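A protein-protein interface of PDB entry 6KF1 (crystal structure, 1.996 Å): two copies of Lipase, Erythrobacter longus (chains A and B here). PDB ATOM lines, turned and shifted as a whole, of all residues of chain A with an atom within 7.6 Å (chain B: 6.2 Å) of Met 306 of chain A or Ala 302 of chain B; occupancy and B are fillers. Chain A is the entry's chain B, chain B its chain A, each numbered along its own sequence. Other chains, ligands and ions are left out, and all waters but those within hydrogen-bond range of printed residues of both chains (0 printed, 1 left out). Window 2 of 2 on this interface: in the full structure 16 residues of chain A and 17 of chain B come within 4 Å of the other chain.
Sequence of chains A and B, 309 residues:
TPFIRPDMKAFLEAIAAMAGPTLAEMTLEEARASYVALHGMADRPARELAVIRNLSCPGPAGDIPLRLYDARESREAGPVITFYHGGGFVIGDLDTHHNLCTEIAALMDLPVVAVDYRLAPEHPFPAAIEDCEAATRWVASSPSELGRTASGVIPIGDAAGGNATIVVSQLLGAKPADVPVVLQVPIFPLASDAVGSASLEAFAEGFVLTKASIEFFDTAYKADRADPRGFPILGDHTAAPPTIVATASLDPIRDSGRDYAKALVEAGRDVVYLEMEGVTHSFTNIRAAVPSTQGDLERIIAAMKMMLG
Val 271 of chain A touches Val 272 of chain B. CG of Met 306 of chain B touches O of Ala 302 of chain A, at 3.6 Å. Met 306 of chain A touches Ala 302 of chain B (CG to O, 3.7 Å). Met 306 of chain B touches Met 306 of chain A.
Ala 302 of chain A touches Met 306 of chain B, and with the chains exchanged Met 306 of chain A touches Ala 302 of chain B. Met 306 of chain A touches its own counterpart, Met 306 of chain B. Of the 4 pairs that touch across the chains among the printed residues, 3 have their exchanged pair printed and touching as well.
Printed residues of chain B within 4 Å of Val 271 of chain A: Val 272 (3.6 Å). Of the printed residues of chain B, Ala 302 of chain A touches Met 306 (3.6 Å). Ala 303 of chain A touches none of the printed residues of chain B. Met 306 of chain A touches just these residues of chain B: Ala 302 (3.7 Å) and Met 306 (2.8 Å). Of chain A, only Met 306 comes within 4 Å of Ala 302 of chain B. Of the printed residues of chain A, Met 306 of chain B touches Ala 302 (3.6 Å) and Met 306 (2.8 Å). The nearest printed residue of chain B that does not touch Ala 302 of chain A is Met 307 of chain B (7.1 Å).
Hydrophobic or aromatic side chains of chain B that line the printed part of chain A: Met 306. Among the printed residues, 4 pairs touch across the chains.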
ATOM      1  N   MET A 108      -4.899  34.002   8.872  1.00  0.00           N
ATOM      2  CA  MET A 108      -4.664  33.755   7.420  1.00  0.00           C
ATOM      3  C   MET A 108      -4.648  35.056   6.615  1.00  0.00           C
ATOM      4  O   MET A 108      -4.101  35.043   5.510  1.00  0.00           O
ATOM      5  CB  MET A 108      -5.755  32.863   6.851  1.00  0.00           C
ATOM      6  CG  MET A 108      -5.705  31.454   7.351  1.00  0.00           C
ATOM      7  SD  MET A 108      -4.196  30.582   6.857  1.00  0.00           S
ATOM      8  CE  MET A 108      -4.229  30.816   5.079  1.00  0.00           C
ATOM      9  N   LEU A 183      -7.846  24.304  -1.935  1.00  0.00           N
ATOM     10  CA  LEU A 183      -7.335  23.638  -0.707  1.00  0.00           C
ATOM     11  C   LEU A 183      -8.578  23.276   0.113  1.00  0.00           C
ATOM     12  O   LEU A 183      -9.572  24.044   0.081  1.00  0.00           O
ATOM     13  CB  LEU A 183      -6.427  24.630   0.042  1.00  0.00           C
ATOM     14  CG  LEU A 183      -5.971  24.161   1.423  1.00  0.00           C
ATOM     15  CD1 LEU A 183      -5.044  22.957   1.274  1.00  0.00           C
ATOM     16  CD2 LEU A 183      -5.269  25.292   2.173  1.00  0.00           C
ATOM     17  N   ILE A 244      -5.407  19.288   3.758  1.00  0.00           N
ATOM     18  CA  ILE A 244      -4.787  19.211   5.090  1.00  0.00           C
ATOM     19  C   ILE A 244      -5.793  18.483   5.965  1.00  0.00           C
ATOM     20  O   ILE A 244      -6.915  19.010   6.133  1.00  0.00           O
ATOM     21  CB  ILE A 244      -4.422  20.564   5.683  1.00  0.00           C
ATOM     22  CG1 ILE A 244      -3.339  21.281   4.857  1.00  0.00           C
ATOM     23  CG2 ILE A 244      -3.930  20.411   7.109  1.00  0.00           C
ATOM     24  CD1 ILE A 244      -3.388  22.740   5.067  1.00  0.00           C
ATOM     25  N   VAL A 271      -1.359  15.655   0.376  1.00  0.00           N
ATOM     26  CA  VAL A 271      -2.060  15.776   1.678  1.00  0.00           C
ATOM     27  C   VAL A 271      -1.056  15.996   2.786  1.00  0.00           C
ATOM     28  O   VAL A 271       0.046  15.437   2.734  1.00  0.00           O
ATOM     29  CB  VAL A 271      -2.959  14.553   1.916  1.00  0.00           C
ATOM     30  CG1 VAL A 271      -2.264  13.234   1.698  1.00  0.00           C
ATOM     31  CG2 VAL A 271      -3.606  14.630   3.284  1.00  0.00           C
ATOM     32  N   VAL A 272      -1.369  16.942   3.668  1.00  0.00           N
ATOM     33  CA  VAL A 272      -0.664  17.131   4.954  1.00  0.00           C
ATOM     34  C   VAL A 272      -1.539  16.409   5.983  1.00  0.00           C
ATOM     35  O   VAL A 272      -2.721  16.755   6.081  1.00  0.00           O
ATOM     36  CB  VAL A 272      -0.490  18.612   5.303  1.00  0.00           C
ATOM     37  CG1 VAL A 272       0.241  18.771   6.614  1.00  0.00           C
ATOM     38  CG2 VAL A 272       0.188  19.393   4.165  1.00  0.00           C
ATOM     39  N   ILE A 300      -1.968  24.102  11.891  1.00  0.00           N
ATOM     40  CA  ILE A 300      -2.902  24.037  10.755  1.00  0.00           C
ATOM     41  C   ILE A 300      -2.749  25.297   9.895  1.00  0.00           C
ATOM     42  O   ILE A 300      -2.680  25.151   8.647  1.00  0.00           O
ATOM     43  CB  ILE A 300      -4.335  23.802  11.234  1.00  0.00           C
ATOM     44  CG1 ILE A 300      -4.431  22.502  12.047  1.00  0.00           C
ATOM     45  CG2 ILE A 300      -5.255  23.826  10.052  1.00  0.00           C
ATOM     46  CD1 ILE A 300      -5.801  22.275  12.690  1.00  0.00           C
ATOM     47  N   ILE A 301      -2.752  26.473  10.500  1.00  0.00           N
ATOM     48  CA  ILE A 301      -2.578  27.753   9.763  1.00  0.00           C
ATOM     49  C   ILE A 301      -1.272  27.680   8.955  1.00  0.00           C
ATOM     50  O   ILE A 301      -1.339  28.024   7.747  1.00  0.00           O
ATOM     51  CB  ILE A 301      -2.611  28.927  10.758  1.00  0.00           C
ATOM     52  CG1 ILE A 301      -3.993  29.065  11.409  1.00  0.00           C
ATOM     53  CG2 ILE A 301      -2.150  30.223  10.103  1.00  0.00           C
ATOM     54  CD1 ILE A 301      -5.070  29.393  10.410  1.00  0.00           C
ATOM     55  N   ALA A 302      -0.146  27.279   9.556  1.00  0.00           N
ATOM     56  CA  ALA A 302       1.174  27.239   8.880  1.00  0.00           C
ATOM     57  C   ALA A 302       1.063  26.298   7.683  1.00  0.00           C
ATOM     58  O   ALA A 302       1.583  26.650   6.580  1.00  0.00           O
ATOM     59  CB  ALA A 302       2.315  26.840   9.819  1.00  0.00           C
ATOM     60  N   ALA A 303       0.409  25.145   7.852  1.00  0.00           N
ATOM     61  CA  ALA A 303       0.237  24.171   6.758  1.00  0.00           C
ATOM     62  C   ALA A 303      -0.596  24.789   5.636  1.00  0.00           C
ATOM     63  O   ALA A 303      -0.264  24.583   4.456  1.00  0.00           O
ATOM     64  CB  ALA A 303      -0.356  22.865   7.243  1.00  0.00           C
ATOM     65  N   MET A 304      -1.683  25.482   5.969  1.00  0.00           N
ATOM     66  CA  MET A 304      -2.567  26.132   4.976  1.00  0.00           C
ATOM     67  C   MET A 304      -1.765  27.138   4.125  1.00  0.00           C
ATOM     68  O   MET A 304      -1.891  27.119   2.911  1.00  0.00           O
ATOM     69  CB  MET A 304      -3.728  26.844   5.680  1.00  0.00           C
ATOM     70  CG  MET A 304      -4.691  25.876   6.243  1.00  0.00           C
ATOM     71  SD  MET A 304      -5.951  26.676   7.331  1.00  0.00           S
ATOM     72  CE  MET A 304      -6.795  27.686   6.128  1.00  0.00           C
ATOM     73  N   LYS A 305      -0.977  27.978   4.757  1.00  0.00           N
ATOM     74  CA  LYS A 305      -0.122  28.984   4.088  1.00  0.00           C
ATOM     75  C   LYS A 305       0.832  28.280   3.119  1.00  0.00           C
ATOM     76  O   LYS A 305       0.981  28.764   1.974  1.00  0.00           O
ATOM     77  CB  LYS A 305       0.623  29.802   5.127  1.00  0.00           C
ATOM     78  CG  LYS A 305      -0.274  30.788   5.857  1.00  0.00           C
ATOM     79  CD  LYS A 305       0.473  31.613   6.815  1.00  0.00           C
ATOM     80  CE  LYS A 305      -0.415  32.642   7.488  1.00  0.00           C
ATOM     81  NZ  LYS A 305       0.354  33.252   8.582  1.00  0.00           N
ATOM     82  N   MET A 306       1.521  27.237   3.587  1.00  0.00           N
ATOM     83  CA  MET A 306       2.464  26.464   2.729  1.00  0.00           C
ATOM     84  C   MET A 306       1.698  25.883   1.550  1.00  0.00           C
ATOM     85  O   MET A 306       2.194  25.970   0.381  1.00  0.00           O
ATOM     86  CB  MET A 306       3.162  25.381   3.543  1.00  0.00           C
ATOM     87  CG  MET A 306       4.158  24.569   2.745  1.00  0.00           C
ATOM     88  SD  MET A 306       3.408  23.108   2.069  1.00  0.00           S
ATOM     89  CE  MET A 306       3.010  22.011   3.415  1.00  0.00           C
ATOM     90  N   MET A 307       0.515  25.330   1.776  1.00  0.00           N
ATOM     91  CA  MET A 307      -0.206  24.590   0.707  1.00  0.00           C
ATOM     92  C   MET A 307      -0.857  25.558  -0.278  1.00  0.00           C
ATOM     93  O   MET A 307      -1.062  25.137  -1.415  1.00  0.00           O
ATOM     94  CB  MET A 307      -1.243  23.609   1.279  1.00  0.00           C
ATOM     95  CG  MET A 307      -0.609  22.448   2.009  1.00  0.00           C
ATOM     96  SD  MET A 307       0.254  21.268   0.924  1.00  0.00           S
ATOM     97  CE  MET A 307      -1.082  20.197   0.399  1.00  0.00           C
ATOM     98  N   LEU A 308      -1.112  26.811   0.111  1.00  0.00           N
ATOM     99  CA  LEU A 308      -1.611  27.852  -0.823  1.00  0.00           C
ATOM    100  C   LEU A 308      -0.447  28.500  -1.587  1.00  0.00           C
ATOM    101  O   LEU A 308      -0.741  29.132  -2.583  1.00  0.00           O
ATOM    102  CB  LEU A 308      -2.358  28.936  -0.052  1.00  0.00           C
ATOM    103  CG  LEU A 308      -3.658  28.470   0.548  1.00  0.00           C
ATOM    104  CD1 LEU A 308      -4.177  29.553   1.461  1.00  0.00           C
ATOM    105  CD2 LEU A 308      -4.659  28.094  -0.530  1.00  0.00           C
ATOM    106  N   GLY A 309       0.802  28.319  -1.158  1.00  0.00           N
ATOM    107  CA  GLY A 309       1.993  29.073  -1.621  1.00  0.00           C
ATOM    108  C   GLY A 309       1.865  30.544  -1.218  1.00  0.00           C
ATOM    109  O   GLY A 309       2.573  31.309  -1.855  1.00  0.00           O
ATOM    110  N   MET B 108      17.479  26.297   1.559  1.00  0.00           N
ATOM    111  CA  MET B 108      17.077  26.064   2.977  1.00  0.00           C
ATOM    112  C   MET B 108      17.814  27.045   3.886  1.00  0.00           C
ATOM    113  O   MET B 108      17.385  27.213   5.024  1.00  0.00           O
ATOM    114  CB  MET B 108      17.401  24.642   3.448  1.00  0.00           C
ATOM    115  CG  MET B 108      16.467  23.615   2.892  1.00  0.00           C
ATOM    116  SD  MET B 108      14.738  23.922   3.354  1.00  0.00           S
ATOM    117  CE  MET B 108      14.813  23.889   5.127  1.00  0.00           C
ATOM    118  N   VAL B 272       3.675  15.044   5.433  1.00  0.00           N
ATOM    119  CA  VAL B 272       3.383  15.689   4.144  1.00  0.00           C
ATOM    120  C   VAL B 272       3.697  14.690   3.026  1.00  0.00           C
ATOM    121  O   VAL B 272       4.849  14.209   2.933  1.00  0.00           O
ATOM    122  CB  VAL B 272       4.172  16.997   4.006  1.00  0.00           C
ATOM    123  CG1 VAL B 272       3.719  17.720   2.737  1.00  0.00           C
ATOM    124  CG2 VAL B 272       3.996  17.876   5.225  1.00  0.00           C
ATOM    125  N   LEU B 274       3.636  14.505  -0.945  1.00  0.00           N
ATOM    126  CA  LEU B 274       3.593  15.269  -2.226  1.00  0.00           C
ATOM    127  C   LEU B 274       3.892  14.309  -3.367  1.00  0.00           C
ATOM    128  O   LEU B 274       5.003  13.768  -3.428  1.00  0.00           O
ATOM    129  CB  LEU B 274       4.648  16.377  -2.189  1.00  0.00           C
ATOM    130  CG  LEU B 274       4.477  17.385  -1.044  1.00  0.00           C
ATOM    131  CD1 LEU B 274       5.551  18.448  -1.108  1.00  0.00           C
ATOM    132  CD2 LEU B 274       3.106  18.032  -1.093  1.00  0.00           C
ATOM    133  N   LEU B 297      11.130  20.610  -6.824  1.00  0.00           N
ATOM    134  CA  LEU B 297      12.085  20.703  -5.696  1.00  0.00           C
ATOM    135  C   LEU B 297      11.680  21.852  -4.780  1.00  0.00           C
ATOM    136  O   LEU B 297      11.825  21.698  -3.547  1.00  0.00           O
ATOM    137  CB  LEU B 297      13.490  20.927  -6.215  1.00  0.00           C
ATOM    138  CG  LEU B 297      14.548  21.211  -5.163  1.00  0.00           C
ATOM    139  CD1 LEU B 297      14.716  20.040  -4.202  1.00  0.00           C
ATOM    140  CD2 LEU B 297      15.890  21.495  -5.847  1.00  0.00           C
ATOM    141  N   GLU B 298      11.287  22.996  -5.349  1.00  0.00           N
ATOM    142  CA  GLU B 298      10.917  24.203  -4.529  1.00  0.00           C
ATOM    143  C   GLU B 298       9.716  23.897  -3.626  1.00  0.00           C
ATOM    144  O   GLU B 298       9.686  24.433  -2.487  1.00  0.00           O
ATOM    145  CB  GLU B 298      10.741  25.427  -5.424  1.00  0.00           C
ATOM    146  CG  GLU B 298      12.102  25.883  -5.941  1.00  0.00           C
ATOM    147  CD  GLU B 298      12.027  26.890  -7.068  1.00  0.00           C
ATOM    148  OE1 GLU B 298      10.939  27.086  -7.562  1.00  0.00           O
ATOM    149  OE2 GLU B 298      13.085  27.456  -7.410  1.00  0.00           O
ATOM    150  N   ARG B 299       8.813  23.023  -4.063  1.00  0.00           N
ATOM    151  CA  ARG B 299       7.670  22.563  -3.224  1.00  0.00           C
ATOM    152  C   ARG B 299       8.162  21.742  -2.019  1.00  0.00           C
ATOM    153  O   ARG B 299       7.631  21.941  -0.907  1.00  0.00           O
ATOM    154  CB  ARG B 299       6.630  21.811  -4.034  1.00  0.00           C
ATOM    155  CG  ARG B 299       5.945  22.707  -5.062  1.00  0.00           C
ATOM    156  CD  ARG B 299       4.898  21.901  -5.823  1.00  0.00           C
ATOM    157  NE  ARG B 299       3.879  21.450  -4.896  1.00  0.00           N
ATOM    158  CZ  ARG B 299       3.106  20.391  -5.053  1.00  0.00           C
ATOM    159  NH1 ARG B 299       3.187  19.661  -6.154  1.00  0.00           N
ATOM    160  NH2 ARG B 299       2.194  20.124  -4.131  1.00  0.00           N
ATOM    161  N   ILE B 300       9.176  20.888  -2.207  1.00  0.00           N
ATOM    162  CA  ILE B 300       9.771  20.100  -1.113  1.00  0.00           C
ATOM    163  C   ILE B 300      10.394  21.061  -0.123  1.00  0.00           C
ATOM    164  O   ILE B 300      10.115  20.924   1.068  1.00  0.00           O
ATOM    165  CB  ILE B 300      10.771  19.068  -1.661  1.00  0.00           C
ATOM    166  CG1 ILE B 300      10.044  18.105  -2.594  1.00  0.00           C
ATOM    167  CG2 ILE B 300      11.458  18.409  -0.498  1.00  0.00           C
ATOM    168  CD1 ILE B 300      10.938  17.094  -3.324  1.00  0.00           C
ATOM    169  N   ILE B 301      11.121  22.057  -0.603  1.00  0.00           N
ATOM    170  CA  ILE B 301      11.804  23.052   0.258  1.00  0.00           C
ATOM    171  C   ILE B 301      10.734  23.805   1.081  1.00  0.00           C
ATOM    172  O   ILE B 301      10.971  24.029   2.274  1.00  0.00           O
ATOM    173  CB  ILE B 301      12.621  24.027  -0.606  1.00  0.00           C
ATOM    174  CG1 ILE B 301      13.802  23.323  -1.276  1.00  0.00           C
ATOM    175  CG2 ILE B 301      13.061  25.250   0.199  1.00  0.00           C
ATOM    176  CD1 ILE B 301      14.894  22.817  -0.349  1.00  0.00           C
ATOM    177  N   ALA B 302       9.667  24.242   0.446  1.00  0.00           N
ATOM    178  CA  ALA B 302       8.581  24.979   1.131  1.00  0.00           C
ATOM    179  C   ALA B 302       8.000  24.076   2.239  1.00  0.00           C
ATOM    180  O   ALA B 302       7.807  24.586   3.331  1.00  0.00           O
ATOM    181  CB  ALA B 302       7.495  25.393   0.156  1.00  0.00           C
ATOM    182  N   ALA B 303       7.738  22.790   1.962  1.00  0.00           N
ATOM    183  CA  ALA B 303       7.228  21.808   2.949  1.00  0.00           C
ATOM    184  C   ALA B 303       8.230  21.651   4.095  1.00  0.00           C
ATOM    185  O   ALA B 303       7.837  21.594   5.322  1.00  0.00           O
ATOM    186  CB  ALA B 303       6.915  20.465   2.269  1.00  0.00           C
ATOM    187  N   MET B 304       9.523  21.590   3.788  1.00  0.00           N
ATOM    188  CA  MET B 304      10.579  21.464   4.829  1.00  0.00           C
ATOM    189  C   MET B 304      10.559  22.670   5.778  1.00  0.00           C
ATOM    190  O   MET B 304      10.609  22.476   7.017  1.00  0.00           O
ATOM    191  CB  MET B 304      11.979  21.311   4.206  1.00  0.00           C
ATOM    192  CG  MET B 304      12.125  19.958   3.481  1.00  0.00           C
ATOM    193  SD  MET B 304      13.636  19.869   2.472  1.00  0.00           S
ATOM    194  CE  MET B 304      14.926  20.046   3.687  1.00  0.00           C
ATOM    195  N   LYS B 305      10.515  23.873   5.232  1.00  0.00           N
ATOM    196  CA  LYS B 305      10.465  25.110   6.050  1.00  0.00           C
ATOM    197  C   LYS B 305       9.211  25.105   6.942  1.00  0.00           C
ATOM    198  O   LYS B 305       9.369  25.425   8.122  1.00  0.00           O
ATOM    199  CB  LYS B 305      10.540  26.324   5.160  1.00  0.00           C
ATOM    200  CG  LYS B 305      11.882  26.518   4.490  1.00  0.00           C
ATOM    201  CD  LYS B 305      11.879  27.753   3.633  1.00  0.00           C
ATOM    202  CE  LYS B 305      13.153  27.969   2.869  1.00  0.00           C
ATOM    203  NZ  LYS B 305      13.996  29.005   3.480  1.00  0.00           N
ATOM    204  N   MET B 306       8.048  24.699   6.422  1.00  0.00           N
ATOM    205  CA  MET B 306       6.818  24.657   7.221  1.00  0.00           C
ATOM    206  C   MET B 306       7.025  23.622   8.349  1.00  0.00           C
ATOM    207  O   MET B 306       6.703  23.919   9.505  1.00  0.00           O
ATOM    208  CB  MET B 306       5.607  24.381   6.329  1.00  0.00           C
ATOM    209  CG  MET B 306       4.289  24.320   7.066  1.00  0.00           C
ATOM    210  SD  MET B 306       3.937  22.627   7.619  1.00  0.00           S
ATOM    211  CE  MET B 306       3.536  21.685   6.171  1.00  0.00           C
ATOM    212  N   MET B 307       7.563  22.440   8.058  1.00  0.00           N
ATOM    213  CA  MET B 307       7.574  21.329   9.047  1.00  0.00           C
ATOM    214  C   MET B 307       8.664  21.604  10.080  1.00  0.00           C
ATOM    215  O   MET B 307       8.536  21.054  11.174  1.00  0.00           O
ATOM    216  CB  MET B 307       7.770  19.963   8.394  1.00  0.00           C
ATOM    217  CG  MET B 307       6.603  19.502   7.571  1.00  0.00           C
ATOM    218  SD  MET B 307       5.090  19.121   8.507  1.00  0.00           S
ATOM    219  CE  MET B 307       5.495  17.462   9.055  1.00  0.00           C
